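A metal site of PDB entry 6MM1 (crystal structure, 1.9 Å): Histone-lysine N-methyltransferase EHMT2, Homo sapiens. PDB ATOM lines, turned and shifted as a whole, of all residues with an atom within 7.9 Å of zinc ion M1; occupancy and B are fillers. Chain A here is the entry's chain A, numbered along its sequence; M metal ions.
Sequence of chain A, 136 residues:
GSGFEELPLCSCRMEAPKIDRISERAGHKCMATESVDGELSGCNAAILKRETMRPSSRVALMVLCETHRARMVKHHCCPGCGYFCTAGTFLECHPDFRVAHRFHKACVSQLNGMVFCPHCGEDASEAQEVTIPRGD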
ATOM      1  N   CYS A  10      12.876 -36.320  26.428  1.00  0.00           N
ATOM      2  CA  CYS A  10      14.285 -36.178  26.099  1.00  0.00           C
ATOM      3  C   CYS A  10      15.143 -36.135  27.347  1.00  0.00           C
ATOM      4  O   CYS A  10      14.660 -35.930  28.455  1.00  0.00           O
ATOM      5  CB  CYS A  10      14.526 -34.899  25.288  1.00  0.00           C
ATOM      6  SG  CYS A  10      14.193 -33.389  26.284  1.00  0.00           S
ATOM      7  N   HIS A  75      17.268 -27.524  24.157  1.00  0.00           N
ATOM      8  CA  HIS A  75      16.520 -28.480  23.355  1.00  0.00           C
ATOM      9  C   HIS A  75      16.676 -28.199  21.867  1.00  0.00           C
ATOM     10  O   HIS A  75      15.747 -28.359  21.090  1.00  0.00           O
ATOM     11  CB  HIS A  75      15.042 -28.509  23.756  1.00  0.00           C
ATOM     12  CG  HIS A  75      14.809 -28.892  25.187  1.00  0.00           C
ATOM     13  ND1 HIS A  75      15.050 -30.161  25.672  1.00  0.00           N
ATOM     14  CD2 HIS A  75      14.368 -28.167  26.239  1.00  0.00           C
ATOM     15  CE1 HIS A  75      14.753 -30.205  26.959  1.00  0.00           C
ATOM     16  NE2 HIS A  75      14.325 -29.006  27.322  1.00  0.00           N
ATOM     17  N   GLU A  92       9.798 -26.842  15.127  1.00  0.00           N
ATOM     18  CA  GLU A  92       9.920 -26.278  16.460  1.00  0.00           C
ATOM     19  C   GLU A  92       8.580 -26.386  17.176  1.00  0.00           C
ATOM     20  O   GLU A  92       7.551 -25.986  16.634  1.00  0.00           O
ATOM     21  CB  GLU A  92      10.353 -24.816  16.416  1.00  0.00           C
ATOM     22  CG  GLU A  92      11.837 -24.610  16.291  1.00  0.00           C
ATOM     23  CD  GLU A  92      12.262 -23.188  16.620  1.00  0.00           C
ATOM     24  OE1 GLU A  92      13.482 -22.932  16.631  1.00  0.00           O
ATOM     25  OE2 GLU A  92      11.377 -22.335  16.860  1.00  0.00           O
ATOM     26  N   CYS A  93       8.622 -26.951  18.373  1.00  0.00           N
ATOM     27  CA  CYS A  93       7.504 -26.969  19.300  1.00  0.00           C
ATOM     28  C   CYS A  93       7.717 -25.813  20.278  1.00  0.00           C
ATOM     29  O   CYS A  93       8.850 -25.554  20.690  1.00  0.00           O
ATOM     30  CB  CYS A  93       7.468 -28.335  20.007  1.00  0.00           C
ATOM     31  SG  CYS A  93       6.653 -28.526  21.603  1.00  0.00           S
ATOM     32  N   HIS A  94       6.637 -25.078  20.608  1.00  0.00           N
ATOM     33  CA  HIS A  94       6.739 -23.870  21.416  1.00  0.00           C
ATOM     34  C   HIS A  94       5.882 -24.009  22.678  1.00  0.00           C
ATOM     35  O   HIS A  94       4.738 -23.533  22.723  1.00  0.00           O
ATOM     36  CB  HIS A  94       6.320 -22.629  20.626  1.00  0.00           C
ATOM     37  CG  HIS A  94       7.250 -22.305  19.495  1.00  0.00           C
ATOM     38  ND1 HIS A  94       6.807 -22.005  18.229  1.00  0.00           N
ATOM     39  CD2 HIS A  94       8.596 -22.227  19.446  1.00  0.00           C
ATOM     40  CE1 HIS A  94       7.836 -21.753  17.441  1.00  0.00           C
ATOM     41  NE2 HIS A  94       8.941 -21.879  18.168  1.00  0.00           N
ATOM     42  N   PRO A  95       6.396 -24.654  23.720  1.00  0.00           N
ATOM     43  CA  PRO A  95       5.593 -24.884  24.920  1.00  0.00           C
ATOM     44  C   PRO A  95       5.409 -23.660  25.802  1.00  0.00           C
ATOM     45  O   PRO A  95       4.509 -23.648  26.651  1.00  0.00           O
ATOM     46  CB  PRO A  95       6.370 -25.974  25.660  1.00  0.00           C
ATOM     47  CG  PRO A  95       7.781 -25.720  25.266  1.00  0.00           C
ATOM     48  CD  PRO A  95       7.726 -25.277  23.825  1.00  0.00           C
ATOM     49  N   VAL A  99      10.707 -20.494  24.409  1.00  0.00           N
ATOM     50  CA  VAL A  99      11.182 -21.880  24.507  1.00  0.00           C
ATOM     51  C   VAL A  99      10.855 -22.562  23.181  1.00  0.00           C
ATOM     52  O   VAL A  99       9.720 -22.474  22.703  1.00  0.00           O
ATOM     53  CB  VAL A  99      10.538 -22.638  25.683  1.00  0.00           C
ATOM     54  CG1 VAL A  99      11.079 -24.067  25.756  1.00  0.00           C
ATOM     55  CG2 VAL A  99      10.818 -21.918  26.995  1.00  0.00           C
ATOM     56  N   ALA A 100      11.861 -23.211  22.601  1.00  0.00           N
ATOM     57  CA  ALA A 100      11.715 -23.932  21.337  1.00  0.00           C
ATOM     58  C   ALA A 100      12.348 -25.297  21.473  1.00  0.00           C
ATOM     59  O   ALA A 100      13.520 -25.396  21.843  1.00  0.00           O
ATOM     60  CB  ALA A 100      12.381 -23.161  20.187  1.00  0.00           C
ATOM     61  N   HIS A 101      11.573 -26.339  21.203  1.00  0.00           N
ATOM     62  CA  HIS A 101      12.075 -27.701  21.079  1.00  0.00           C
ATOM     63  C   HIS A 101      12.257 -27.991  19.602  1.00  0.00           C
ATOM     64  O   HIS A 101      11.268 -27.994  18.852  1.00  0.00           O
ATOM     65  CB  HIS A 101      11.081 -28.691  21.686  1.00  0.00           C
ATOM     66  CG  HIS A 101      10.788 -28.457  23.139  1.00  0.00           C
ATOM     67  ND1 HIS A 101       9.655 -28.941  23.747  1.00  0.00           N
ATOM     68  CD2 HIS A 101      11.498 -27.828  24.104  1.00  0.00           C
ATOM     69  CE1 HIS A 101       9.661 -28.608  25.028  1.00  0.00           C
ATOM     70  NE2 HIS A 101      10.777 -27.929  25.266  1.00  0.00           N
ATOM     71  N   ARG A 102      13.494 -28.232  19.165  1.00  0.00           N
ATOM     72  CA  ARG A 102      13.774 -28.392  17.755  1.00  0.00           C
ATOM     73  C   ARG A 102      13.931 -29.859  17.428  1.00  0.00           C
ATOM     74  O   ARG A 102      14.535 -30.623  18.192  1.00  0.00           O
ATOM     75  CB  ARG A 102      15.039 -27.636  17.339  1.00  0.00           C
ATOM     76  CG  ARG A 102      14.996 -26.155  17.606  1.00  0.00           C
ATOM     77  CD  ARG A 102      16.240 -25.468  17.065  1.00  0.00           C
ATOM     78  NE  ARG A 102      16.103 -24.019  17.128  1.00  0.00           N
ATOM     79  CZ  ARG A 102      17.065 -23.163  16.821  1.00  0.00           C
ATOM     80  NH1 ARG A 102      18.259 -23.605  16.443  1.00  0.00           N
ATOM     81  NH2 ARG A 102      16.840 -21.855  16.921  1.00  0.00           N
ATOM     82  N   PHE A 103      13.418 -30.257  16.265  1.00  0.00           N
ATOM     83  CA  PHE A 103      13.535 -31.646  15.843  1.00  0.00           C
ATOM     84  C   PHE A 103      13.235 -31.734  14.351  1.00  0.00           C
ATOM     85  O   PHE A 103      12.665 -30.815  13.768  1.00  0.00           O
ATOM     86  CB  PHE A 103      12.605 -32.551  16.651  1.00  0.00           C
ATOM     87  CG  PHE A 103      11.170 -32.091  16.690  1.00  0.00           C
ATOM     88  CD1 PHE A 103      10.750 -31.125  17.579  1.00  0.00           C
ATOM     89  CD2 PHE A 103      10.237 -32.649  15.834  1.00  0.00           C
ATOM     90  CE1 PHE A 103       9.437 -30.704  17.607  1.00  0.00           C
ATOM     91  CE2 PHE A 103       8.913 -32.247  15.867  1.00  0.00           C
ATOM     92  CZ  PHE A 103       8.517 -31.260  16.747  1.00  0.00           C
ATOM     93  N   PHE A 116       4.358 -36.793  17.921  1.00  0.00           N
ATOM     94  CA  PHE A 116       4.523 -35.960  19.103  1.00  0.00           C
ATOM     95  C   PHE A 116       5.938 -35.390  19.144  1.00  0.00           C
ATOM     96  O   PHE A 116       6.872 -35.951  18.563  1.00  0.00           O
ATOM     97  CB  PHE A 116       4.258 -36.740  20.389  1.00  0.00           C
ATOM     98  CG  PHE A 116       2.879 -37.347  20.447  1.00  0.00           C
ATOM     99  CD1 PHE A 116       2.645 -38.613  19.937  1.00  0.00           C
ATOM    100  CD2 PHE A 116       1.826 -36.645  20.997  1.00  0.00           C
ATOM    101  CE1 PHE A 116       1.374 -39.176  20.005  1.00  0.00           C
ATOM    102  CE2 PHE A 116       0.550 -37.198  21.055  1.00  0.00           C
ATOM    103  CZ  PHE A 116       0.335 -38.465  20.558  1.00  0.00           C
ATOM    104  N   CYS A 117       6.079 -34.256  19.849  1.00  0.00           N
ATOM    105  CA  CYS A 117       7.391 -33.663  20.053  1.00  0.00           C
ATOM    106  C   CYS A 117       8.272 -34.660  20.784  1.00  0.00           C
ATOM    107  O   CYS A 117       7.877 -35.168  21.847  1.00  0.00           O
ATOM    108  CB  CYS A 117       7.282 -32.352  20.854  1.00  0.00           C
ATOM    109  SG  CYS A 117       8.889 -31.606  21.363  1.00  0.00           S
ATOM    110  N   PRO A 118       9.453 -34.995  20.265  1.00  0.00           N
ATOM    111  CA  PRO A 118      10.330 -35.949  20.956  1.00  0.00           C
ATOM    112  C   PRO A 118      11.026 -35.373  22.168  1.00  0.00           C
ATOM    113  O   PRO A 118      11.761 -36.106  22.839  1.00  0.00           O
ATOM    114  CB  PRO A 118      11.343 -36.341  19.881  1.00  0.00           C
ATOM    115  CG  PRO A 118      11.429 -35.146  19.036  1.00  0.00           C
ATOM    116  CD  PRO A 118      10.052 -34.507  19.006  1.00  0.00           C
ATOM    117  N   HIS A 119      10.877 -34.078  22.463  1.00  0.00           N
ATOM    118  CA  HIS A 119      11.395 -33.580  23.738  1.00  0.00           C
ATOM    119  C   HIS A 119      10.369 -33.758  24.843  1.00  0.00           C
ATOM    120  O   HIS A 119      10.647 -34.412  25.863  1.00  0.00           O
ATOM    121  CB  HIS A 119      11.817 -32.112  23.662  1.00  0.00           C
ATOM    122  CG  HIS A 119      12.852 -31.832  22.611  1.00  0.00           C
ATOM    123  ND1 HIS A 119      14.192 -31.724  22.924  1.00  0.00           N
ATOM    124  CD2 HIS A 119      12.758 -31.602  21.282  1.00  0.00           C
ATOM    125  CE1 HIS A 119      14.886 -31.450  21.825  1.00  0.00           C
ATOM    126  NE2 HIS A 119      14.031 -31.367  20.819  1.00  0.00           N
ATOM    127  N   CYS A 120       9.162 -33.195  24.648  1.00  0.00           N
ATOM    128  CA  CYS A 120       8.202 -32.989  25.711  1.00  0.00           C
ATOM    129  C   CYS A 120       6.901 -33.759  25.535  1.00  0.00           C
ATOM    130  O   CYS A 120       6.095 -33.770  26.459  1.00  0.00           O
ATOM    131  CB  CYS A 120       7.862 -31.498  25.838  1.00  0.00           C
ATOM    132  SG  CYS A 120       6.750 -30.902  24.526  1.00  0.00           S
ATOM    133  N   GLY A 121       6.671 -34.354  24.374  1.00  0.00           N
ATOM    134  CA  GLY A 121       5.490 -35.160  24.157  1.00  0.00           C
ATOM    135  C   GLY A 121       4.250 -34.412  23.695  1.00  0.00           C
ATOM    136  O   GLY A 121       3.185 -35.033  23.532  1.00  0.00           O
ATOM    137  N   GLU A 122       4.342 -33.105  23.466  1.00  0.00           N
ATOM    138  CA  GLU A 122       3.206 -32.376  22.921  1.00  0.00           C
ATOM    139  C   GLU A 122       2.903 -32.823  21.493  1.00  0.00           C
ATOM    140  O   GLU A 122       3.799 -33.243  20.755  1.00  0.00           O
ATOM    141  CB  GLU A 122       3.475 -30.869  22.972  1.00  0.00           C
ATOM    142  CG  GLU A 122       2.319 -30.009  22.473  1.00  0.00           C
ATOM    143  CD  GLU A 122       1.082 -30.133  23.326  1.00  0.00           C
ATOM    144  OE1 GLU A 122       0.398 -31.188  23.276  1.00  0.00           O
ATOM    145  OE2 GLU A 122       0.767 -29.159  24.051  1.00  0.00           O
ATOM    146  N   ASP A 123       1.616 -32.741  21.102  1.00  0.00           N
ATOM    147  CA  ASP A 123       1.217 -33.126  19.755  1.00  0.00           C
ATOM    148  C   ASP A 123       2.044 -32.363  18.712  1.00  0.00           C
ATOM    149  O   ASP A 123       2.183 -31.141  18.791  1.00  0.00           O
ATOM    150  CB  ASP A 123      -0.276 -32.860  19.558  1.00  0.00           C
ATOM    151  CG  ASP A 123      -0.705 -32.944  18.084  1.00  0.00           C
ATOM    152  OD1 ASP A 123      -0.581 -34.033  17.485  1.00  0.00           O
ATOM    153  OD2 ASP A 123      -1.168 -31.921  17.536  1.00  0.00           O
ATOM    154  N   ALA A 127       3.398 -28.377  15.683  1.00  0.00           N
ATOM    155  CA  ALA A 127       4.755 -27.900  15.489  1.00  0.00           C
ATOM    156  C   ALA A 127       4.861 -27.005  14.273  1.00  0.00           C
ATOM    157  O   ALA A 127       4.318 -27.316  13.200  1.00  0.00           O
ATOM    158  CB  ALA A 127       5.721 -29.076  15.361  1.00  0.00           C
HETATM  159 ZN    ZN M   1       8.045 -30.013  22.825  1.00  0.00          ZN
HETATM  160 ZN    ZN M   2      15.102 -31.904  24.846  1.00  0.00          ZN
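The side-chain sulfur (SG) of Cys 120 lies close to the backbone NH (N) of Glu 122 (3.4 Å).
The side-chain sulfur (SG) of Cys 117 sits close to the backbone NH (N) of His 119 (3.4 Å).
The backbone NH of Cys 117 lies within hydrogen-bond range of the backbone carbonyl oxygen of Glu 122 (2.7 Å).
Four residues have an atom within 4 Å of zinc ion M1: Cys 93, His 101, Cys 117 and Cys 120.
The nearest printed residue that does not touch zinc ion M1 is His 119 (4.4 Å).
Zinc ion M1 is bound by ND1 of His 101, at 2.1 Å.
Zinc ion M1 is bound by SG of Cys 120.
Zinc ion M1 is bound by SG of Cys 117.
Zinc ion M1 is bound by SG of Cys 93.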
